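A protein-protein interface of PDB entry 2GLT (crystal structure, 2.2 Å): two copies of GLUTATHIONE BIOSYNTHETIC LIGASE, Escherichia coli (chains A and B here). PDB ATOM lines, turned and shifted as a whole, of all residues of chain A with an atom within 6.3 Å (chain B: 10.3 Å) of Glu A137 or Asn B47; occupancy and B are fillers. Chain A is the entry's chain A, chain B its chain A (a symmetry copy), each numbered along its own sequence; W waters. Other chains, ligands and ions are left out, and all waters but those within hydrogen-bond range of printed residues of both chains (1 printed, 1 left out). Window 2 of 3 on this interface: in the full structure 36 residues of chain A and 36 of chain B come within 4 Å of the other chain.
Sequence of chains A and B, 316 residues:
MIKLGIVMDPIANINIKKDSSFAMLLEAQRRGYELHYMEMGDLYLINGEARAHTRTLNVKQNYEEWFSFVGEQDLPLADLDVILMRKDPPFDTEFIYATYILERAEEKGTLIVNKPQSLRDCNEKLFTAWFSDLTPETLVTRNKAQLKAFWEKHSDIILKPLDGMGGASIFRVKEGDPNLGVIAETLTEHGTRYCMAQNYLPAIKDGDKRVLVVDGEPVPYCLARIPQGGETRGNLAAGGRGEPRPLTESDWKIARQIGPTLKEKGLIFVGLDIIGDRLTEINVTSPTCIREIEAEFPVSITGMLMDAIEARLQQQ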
ATOM      1  N   ALA A 129     -16.152  -0.142  31.096  1.00  0.00           N
ATOM      2  CA  ALA A 129     -14.814  -0.651  31.354  1.00  0.00           C
ATOM      3  C   ALA A 129     -14.114  -0.070  32.583  1.00  0.00           C
ATOM      4  O   ALA A 129     -13.175  -0.681  33.109  1.00  0.00           O
ATOM      5  CB  ALA A 129     -13.899  -0.383  30.172  1.00  0.00           C
ATOM      6  N   SER A 132     -15.729  -2.344  36.066  1.00  0.00           N
ATOM      7  CA  SER A 132     -15.669  -3.738  35.676  1.00  0.00           C
ATOM      8  C   SER A 132     -16.172  -4.733  36.716  1.00  0.00           C
ATOM      9  O   SER A 132     -16.589  -5.836  36.390  1.00  0.00           O
ATOM     10  CB  SER A 132     -14.219  -4.066  35.280  1.00  0.00           C
ATOM     11  OG  SER A 132     -13.316  -3.029  35.674  1.00  0.00           O
ATOM     12  N   THR A 135     -20.100  -4.788  35.977  1.00  0.00           N
ATOM     13  CA  THR A 135     -20.655  -5.142  34.686  1.00  0.00           C
ATOM     14  C   THR A 135     -20.601  -6.649  34.398  1.00  0.00           C
ATOM     15  O   THR A 135     -19.937  -7.418  35.117  1.00  0.00           O
ATOM     16  CB  THR A 135     -19.872  -4.284  33.630  1.00  0.00           C
ATOM     17  OG1 THR A 135     -18.491  -4.581  33.744  1.00  0.00           O
ATOM     18  CG2 THR A 135     -19.969  -2.774  33.889  1.00  0.00           C
ATOM     19  N   PRO A 136     -21.303  -7.162  33.381  1.00  0.00           N
ATOM     20  CA  PRO A 136     -21.080  -8.520  32.882  1.00  0.00           C
ATOM     21  C   PRO A 136     -19.723  -8.739  32.226  1.00  0.00           C
ATOM     22  O   PRO A 136     -18.952  -7.802  32.045  1.00  0.00           O
ATOM     23  CB  PRO A 136     -22.228  -8.765  31.925  1.00  0.00           C
ATOM     24  CG  PRO A 136     -22.741  -7.388  31.562  1.00  0.00           C
ATOM     25  CD  PRO A 136     -22.505  -6.551  32.807  1.00  0.00           C
ATOM     26  N   GLU A 137     -19.373  -9.964  31.845  1.00  0.00           N
ATOM     27  CA  GLU A 137     -18.140 -10.261  31.132  1.00  0.00           C
ATOM     28  C   GLU A 137     -18.260  -9.590  29.792  1.00  0.00           C
ATOM     29  O   GLU A 137     -19.238  -9.803  29.089  1.00  0.00           O
ATOM     30  CB  GLU A 137     -18.004 -11.744  30.924  1.00  0.00           C
ATOM     31  CG  GLU A 137     -17.860 -12.514  32.197  1.00  0.00           C
ATOM     32  CD  GLU A 137     -16.430 -12.749  32.665  1.00  0.00           C
ATOM     33  OE1 GLU A 137     -15.585 -13.297  31.926  1.00  0.00           O
ATOM     34  OE2 GLU A 137     -16.205 -12.381  33.813  1.00  0.00           O
ATOM     35  N   THR A 138     -17.264  -8.780  29.465  1.00  0.00           N
ATOM     36  CA  THR A 138     -17.332  -7.920  28.291  1.00  0.00           C
ATOM     37  C   THR A 138     -16.047  -8.054  27.507  1.00  0.00           C
ATOM     38  O   THR A 138     -14.977  -7.845  28.098  1.00  0.00           O
ATOM     39  CB  THR A 138     -17.459  -6.455  28.701  1.00  0.00           C
ATOM     40  OG1 THR A 138     -18.563  -6.359  29.564  1.00  0.00           O
ATOM     41  CG2 THR A 138     -17.676  -5.510  27.517  1.00  0.00           C
ATOM     42  N   LEU A 139     -16.141  -8.359  26.205  1.00  0.00           N
ATOM     43  CA  LEU A 139     -14.990  -8.349  25.324  1.00  0.00           C
ATOM     44  C   LEU A 139     -15.211  -7.288  24.258  1.00  0.00           C
ATOM     45  O   LEU A 139     -16.266  -7.269  23.622  1.00  0.00           O
ATOM     46  CB  LEU A 139     -14.842  -9.731  24.687  1.00  0.00           C
ATOM     47  CG  LEU A 139     -13.891  -9.948  23.526  1.00  0.00           C
ATOM     48  CD1 LEU A 139     -12.460  -9.632  23.924  1.00  0.00           C
ATOM     49  CD2 LEU A 139     -14.040 -11.375  23.054  1.00  0.00           C
ATOM     50  N   PHE A 150     -14.981 -16.484  23.219  1.00  0.00           N
ATOM     51  CA  PHE A 150     -15.710 -15.932  24.337  1.00  0.00           C
ATOM     52  C   PHE A 150     -17.019 -16.726  24.440  1.00  0.00           C
ATOM     53  O   PHE A 150     -17.549 -16.988  25.508  1.00  0.00           O
ATOM     54  CB  PHE A 150     -15.960 -14.458  24.048  1.00  0.00           C
ATOM     55  CG  PHE A 150     -16.576 -13.652  25.192  1.00  0.00           C
ATOM     56  CD1 PHE A 150     -15.777 -13.217  26.243  1.00  0.00           C
ATOM     57  CD2 PHE A 150     -17.936 -13.329  25.199  1.00  0.00           C
ATOM     58  CE1 PHE A 150     -16.341 -12.465  27.286  1.00  0.00           C
ATOM     59  CE2 PHE A 150     -18.483 -12.581  26.245  1.00  0.00           C
ATOM     60  CZ  PHE A 150     -17.696 -12.141  27.290  1.00  0.00           C
ATOM     61  N   LYS A 153     -16.533 -20.134  26.258  1.00  0.00           N
ATOM     62  CA  LYS A 153     -16.458 -20.009  27.694  1.00  0.00           C
ATOM     63  C   LYS A 153     -17.808 -19.685  28.347  1.00  0.00           C
ATOM     64  O   LYS A 153     -18.047 -20.023  29.517  1.00  0.00           O
ATOM     65  CB  LYS A 153     -15.446 -18.911  28.040  1.00  0.00           C
ATOM     66  CG  LYS A 153     -15.281 -18.632  29.545  1.00  0.00           C
ATOM     67  CD  LYS A 153     -14.476 -17.369  29.914  1.00  0.00           C
ATOM     68  CE  LYS A 153     -14.329 -17.175  31.443  1.00  0.00           C
ATOM     69  NZ  LYS A 153     -13.700 -15.911  31.823  1.00  0.00           N
ATOM     70  N   HIS A 154     -18.694 -18.984  27.627  1.00  0.00           N
ATOM     71  CA  HIS A 154     -19.907 -18.505  28.255  1.00  0.00           C
ATOM     72  C   HIS A 154     -21.199 -19.121  27.751  1.00  0.00           C
ATOM     73  O   HIS A 154     -22.246 -19.000  28.403  1.00  0.00           O
ATOM     74  CB  HIS A 154     -19.966 -16.978  28.114  1.00  0.00           C
ATOM     75  CG  HIS A 154     -18.872 -16.291  28.926  1.00  0.00           C
ATOM     76  ND1 HIS A 154     -18.858 -16.039  30.242  1.00  0.00           N
ATOM     77  CD2 HIS A 154     -17.668 -15.831  28.422  1.00  0.00           C
ATOM     78  CE1 HIS A 154     -17.715 -15.456  30.531  1.00  0.00           C
ATOM     79  NE2 HIS A 154     -16.994 -15.340  29.439  1.00  0.00           N
ATOM     80  N   ALA A 197     -19.037  -7.995  23.047  1.00  0.00           N
ATOM     81  CA  ALA A 197     -19.665  -9.270  23.392  1.00  0.00           C
ATOM     82  C   ALA A 197     -19.757  -9.199  24.889  1.00  0.00           C
ATOM     83  O   ALA A 197     -18.886  -8.658  25.571  1.00  0.00           O
ATOM     84  CB  ALA A 197     -18.773 -10.442  23.025  1.00  0.00           C
ATOM     85  N   GLN A 198     -20.887  -9.624  25.418  1.00  0.00           N
ATOM     86  CA  GLN A 198     -21.087  -9.708  26.855  1.00  0.00           C
ATOM     87  C   GLN A 198     -21.790 -10.998  27.149  1.00  0.00           C
ATOM     88  O   GLN A 198     -22.464 -11.487  26.252  1.00  0.00           O
ATOM     89  CB  GLN A 198     -21.992  -8.691  27.399  1.00  0.00           C
ATOM     90  CG  GLN A 198     -21.384  -7.333  27.349  1.00  0.00           C
ATOM     91  CD  GLN A 198     -22.400  -6.312  27.778  1.00  0.00           C
ATOM     92  OE1 GLN A 198     -23.564  -6.384  27.392  1.00  0.00           O
ATOM     93  NE2 GLN A 198     -21.963  -5.343  28.580  1.00  0.00           N
ATOM     94  N   ASN A 199     -21.717 -11.591  28.338  1.00  0.00           N
ATOM     95  CA  ASN A 199     -22.486 -12.806  28.547  1.00  0.00           C
ATOM     96  C   ASN A 199     -23.961 -12.443  28.727  1.00  0.00           C
ATOM     97  O   ASN A 199     -24.311 -11.392  29.259  1.00  0.00           O
ATOM     98  CB  ASN A 199     -21.971 -13.624  29.777  1.00  0.00           C
ATOM     99  CG  ASN A 199     -21.977 -12.872  31.068  1.00  0.00           C
ATOM    100  OD1 ASN A 199     -21.294 -11.869  31.169  1.00  0.00           O
ATOM    101  ND2 ASN A 199     -22.724 -13.277  32.093  1.00  0.00           N
ATOM    102  N   TYR B  44      -7.465  -5.101  22.224  1.00  0.00           N
ATOM    103  CA  TYR B  44      -8.776  -5.480  22.714  1.00  0.00           C
ATOM    104  C   TYR B  44      -8.891  -5.258  24.212  1.00  0.00           C
ATOM    105  O   TYR B  44      -7.917  -4.948  24.893  1.00  0.00           O
ATOM    106  CB  TYR B  44      -9.100  -6.940  22.356  1.00  0.00           C
ATOM    107  CG  TYR B  44      -8.324  -8.007  23.101  1.00  0.00           C
ATOM    108  CD1 TYR B  44      -7.088  -8.421  22.614  1.00  0.00           C
ATOM    109  CD2 TYR B  44      -8.870  -8.579  24.266  1.00  0.00           C
ATOM    110  CE1 TYR B  44      -6.395  -9.421  23.278  1.00  0.00           C
ATOM    111  CE2 TYR B  44      -8.173  -9.579  24.927  1.00  0.00           C
ATOM    112  CZ  TYR B  44      -6.943  -9.999  24.428  1.00  0.00           C
ATOM    113  OH  TYR B  44      -6.258 -10.998  25.084  1.00  0.00           O
ATOM    114  N   LEU B  45     -10.086  -5.405  24.788  1.00  0.00           N
ATOM    115  CA  LEU B  45     -10.318  -5.051  26.182  1.00  0.00           C
ATOM    116  C   LEU B  45     -11.075  -6.217  26.737  1.00  0.00           C
ATOM    117  O   LEU B  45     -12.099  -6.606  26.182  1.00  0.00           O
ATOM    118  CB  LEU B  45     -11.156  -3.805  26.200  1.00  0.00           C
ATOM    119  CG  LEU B  45     -11.117  -2.831  27.333  1.00  0.00           C
ATOM    120  CD1 LEU B  45      -9.805  -2.090  27.357  1.00  0.00           C
ATOM    121  CD2 LEU B  45     -12.211  -1.803  27.106  1.00  0.00           C
ATOM    122  N   ILE B  46     -10.594  -6.865  27.776  1.00  0.00           N
ATOM    123  CA  ILE B  46     -11.339  -7.966  28.360  1.00  0.00           C
ATOM    124  C   ILE B  46     -11.509  -7.542  29.800  1.00  0.00           C
ATOM    125  O   ILE B  46     -10.565  -7.282  30.527  1.00  0.00           O
ATOM    126  CB  ILE B  46     -10.534  -9.282  28.138  1.00  0.00           C
ATOM    127  CG1 ILE B  46     -11.239 -10.397  28.875  1.00  0.00           C
ATOM    128  CG2 ILE B  46      -9.089  -9.145  28.566  1.00  0.00           C
ATOM    129  CD1 ILE B  46     -12.560 -10.806  28.216  1.00  0.00           C
ATOM    130  N   ASN B  47     -12.782  -7.384  30.165  1.00  0.00           N
ATOM    131  CA  ASN B  47     -13.270  -6.817  31.427  1.00  0.00           C
ATOM    132  C   ASN B  47     -12.468  -5.650  31.955  1.00  0.00           C
ATOM    133  O   ASN B  47     -11.880  -5.702  33.038  1.00  0.00           O
ATOM    134  CB  ASN B  47     -13.343  -7.882  32.500  1.00  0.00           C
ATOM    135  CG  ASN B  47     -14.205  -9.039  32.076  1.00  0.00           C
ATOM    136  OD1 ASN B  47     -15.305  -8.868  31.569  1.00  0.00           O
ATOM    137  ND2 ASN B  47     -13.694 -10.260  32.210  1.00  0.00           N
ATOM    138  N   GLY B  48     -12.419  -4.569  31.160  1.00  0.00           N
ATOM    139  CA  GLY B  48     -11.676  -3.393  31.583  1.00  0.00           C
ATOM    140  C   GLY B  48     -10.170  -3.460  31.318  1.00  0.00           C
ATOM    141  O   GLY B  48      -9.537  -2.418  31.213  1.00  0.00           O
ATOM    142  N   GLU B  49      -9.516  -4.623  31.200  1.00  0.00           N
ATOM    143  CA  GLU B  49      -8.089  -4.701  30.917  1.00  0.00           C
ATOM    144  C   GLU B  49      -7.782  -4.643  29.434  1.00  0.00           C
ATOM    145  O   GLU B  49      -8.341  -5.371  28.612  1.00  0.00           O
ATOM    146  CB  GLU B  49      -7.521  -5.987  31.475  1.00  0.00           C
ATOM    147  CG  GLU B  49      -6.033  -6.137  31.324  1.00  0.00           C
ATOM    148  CD  GLU B  49      -5.518  -7.506  31.733  1.00  0.00           C
ATOM    149  OE1 GLU B  49      -6.088  -8.527  31.326  1.00  0.00           O
ATOM    150  OE2 GLU B  49      -4.524  -7.556  32.467  1.00  0.00           O
ATOM    151  N   ALA B  50      -6.868  -3.699  29.162  1.00  0.00           N
ATOM    152  CA  ALA B  50      -6.305  -3.453  27.841  1.00  0.00           C
ATOM    153  C   ALA B  50      -5.229  -4.478  27.538  1.00  0.00           C
ATOM    154  O   ALA B  50      -4.267  -4.648  28.297  1.00  0.00           O
ATOM    155  CB  ALA B  50      -5.691  -2.049  27.788  1.00  0.00           C
ATOM    156  N   ARG B  51      -5.412  -5.204  26.436  1.00  0.00           N
ATOM    157  CA  ARG B  51      -4.482  -6.222  25.982  1.00  0.00           C
ATOM    158  C   ARG B  51      -4.324  -6.148  24.479  1.00  0.00           C
ATOM    159  O   ARG B  51      -5.075  -5.511  23.723  1.00  0.00           O
ATOM    160  CB  ARG B  51      -4.974  -7.637  26.294  1.00  0.00           C
ATOM    161  CG  ARG B  51      -5.305  -7.995  27.749  1.00  0.00           C
ATOM    162  CD  ARG B  51      -5.305  -9.528  27.758  1.00  0.00           C
ATOM    163  NE  ARG B  51      -4.672  -9.867  28.986  1.00  0.00           N
ATOM    164  CZ  ARG B  51      -3.635 -10.681  29.063  1.00  0.00           C
ATOM    165  NH1 ARG B  51      -3.079 -11.281  28.011  1.00  0.00           N
ATOM    166  NH2 ARG B  51      -3.119 -10.833  30.260  1.00  0.00           N
ATOM    167  N   ILE B 101      -8.983   2.219  24.880  1.00  0.00           N
ATOM    168  CA  ILE B 101      -8.201   1.003  25.195  1.00  0.00           C
ATOM    169  C   ILE B 101      -6.793   1.392  25.670  1.00  0.00           C
ATOM    170  O   ILE B 101      -6.315   0.925  26.715  1.00  0.00           O
ATOM    171  CB  ILE B 101      -8.142   0.086  23.934  1.00  0.00           C
ATOM    172  CG1 ILE B 101      -9.559  -0.375  23.678  1.00  0.00           C
ATOM    173  CG2 ILE B 101      -7.222  -1.138  24.108  1.00  0.00           C
ATOM    174  CD1 ILE B 101      -9.737  -1.119  22.344  1.00  0.00           C
ATOM    175  N   ARG B 104      -6.765   2.730  29.147  1.00  0.00           N
ATOM    176  CA  ARG B 104      -6.834   1.763  30.230  1.00  0.00           C
ATOM    177  C   ARG B 104      -5.452   1.243  30.555  1.00  0.00           C
ATOM    178  O   ARG B 104      -5.128   1.051  31.727  1.00  0.00           O
ATOM    179  CB  ARG B 104      -7.729   0.622  29.849  1.00  0.00           C
ATOM    180  CG  ARG B 104      -9.160   1.132  29.748  1.00  0.00           C
ATOM    181  CD  ARG B 104     -10.083   0.605  30.812  1.00  0.00           C
ATOM    182  NE  ARG B 104     -10.063   1.306  32.065  1.00  0.00           N
ATOM    183  CZ  ARG B 104      -9.937   0.659  33.236  1.00  0.00           C
ATOM    184  NH1 ARG B 104      -9.796  -0.663  33.363  1.00  0.00           N
ATOM    185  NH2 ARG B 104     -10.014   1.362  34.354  1.00  0.00           N
ATOM    186  N   LYS B 108      -2.955   2.021  34.165  1.00  0.00           N
ATOM    187  CA  LYS B 108      -2.151   0.995  34.790  1.00  0.00           C
ATOM    188  C   LYS B 108      -0.662   1.244  34.625  1.00  0.00           C
ATOM    189  O   LYS B 108       0.139   0.355  34.925  1.00  0.00           O
ATOM    190  CB  LYS B 108      -2.513  -0.370  34.220  1.00  0.00           C
ATOM    191  CG  LYS B 108      -3.770  -0.899  34.893  1.00  0.00           C
ATOM    192  CD  LYS B 108      -4.065  -2.333  34.459  1.00  0.00           C
ATOM    193  CE  LYS B 108      -5.497  -2.748  34.850  1.00  0.00           C
ATOM    194  NZ  LYS B 108      -5.948  -3.924  34.114  1.00  0.00           N
HETATM  195  O   HOH W   1     -14.958 -10.150  35.191  1.00  0.00           O
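The backbone carbonyl oxygen (O) of Ala A129 is in hydrogen-bond range of the guanidinium group (NH1) of Arg B104 (3.4 Å). The side-chain amide oxygen (OD1) of Asn B47 sits at hydrogen-bond distance from the backbone NH (N) of Thr A138 (2.9 Å).
O of Ala A129 sits at hydrogen-bond distance from OG of Ser A132 (3.5 Å). O of Ser A132 lies within hydrogen-bond range of OG1 of Thr A135 (3.5 Å). The side-chain carboxylate of Glu A137 is in salt-bridge range of the side-chain amino group of Lys A153, at 3.2 Å. The backbone NH (N) of Leu A139 is in hydrogen-bond range of the backbone carbonyl oxygen (O) of Ala A197, at 2.8 Å. The backbone carbonyl oxygen of Arg B51 is in hydrogen-bond range of the backbone NH of Tyr B44, 2.9 Å away. The backbone carbonyl oxygen of Gly B48 sits at hydrogen-bond distance from the guanidinium group of Arg B104, at 2.8 Å.
Among the printed residues, merely in contact across the chains: Ala A129 with Leu B45 (3.8 Å), Ala A129 with Gly B48 (3.5 Å), Ser A132 with Asn B47 (3.6 Å), Pro A136 with Asn B47 (3.8 Å), Glu A137 with Asn B47 (3.2 Å), Thr A138 with Leu B45 (3.7 Å), Thr A138 with Ile B46 (3.6 Å), Leu A139 with Tyr B44 (3.8 Å) and Leu A139 with Leu B45 (3.5 Å).
Of the printed residues of chain B, Glu A137 touches Asn B47. Of the printed residues of chain A, Asn B47 touches Ser A132, Pro A136, Glu A137 and Thr A138. Of chain B, only Asn B47 comes within 4 Å of Pro A136. Thr A138 touches three residues of chain B. No residue of chain B comes within 4 Å of Asn A199. Of the printed residues of chain A, Arg B104 touches Ala A129. Of the printed residues of chain A, Gly B48 touches Ala A129. Phe A150 touches none of the printed residues of chain B. Lys B108 touches none of the printed residues of chain A. The nearest residue of chain B that does not touch Glu A137 is Ile B46 (5.4 Å). The nearest residue of chain A that does not touch Asn B47 is Ala A129 (5.2 Å). The nearest printed residue of chain A that does not touch Tyr B44 is Thr A138 (7.2 Å).
Along chain A the printed residues that touch a printed residue of chain B span positions 129 to 139. Of the 11 printed residues of chain B, 6 touch a printed residue of chain A. Printed residues of chain B that touch a printed residue of chain A: Tyr B44, Leu B45, Ile B46, Asn B47, Gly B48 and Arg B104. Hydrophobic or aromatic side chains of chain B that line the printed part of chain A: Tyr B44, Leu B45 and Ile B46. Along chain B the printed residues that touch a printed residue of chain A span positions 44 to 104. Among the printed residues, no Asp or Glu carboxylate lies within 4 Å of a Lys or Arg side-chain nitrogen of the other chain.
No position is printed for both chains.
Water W1 bridges the side-chain carboxylate of Glu A137 (2.9 Å) and the side-chain amide nitrogen of Asn B47 (3.2 Å).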
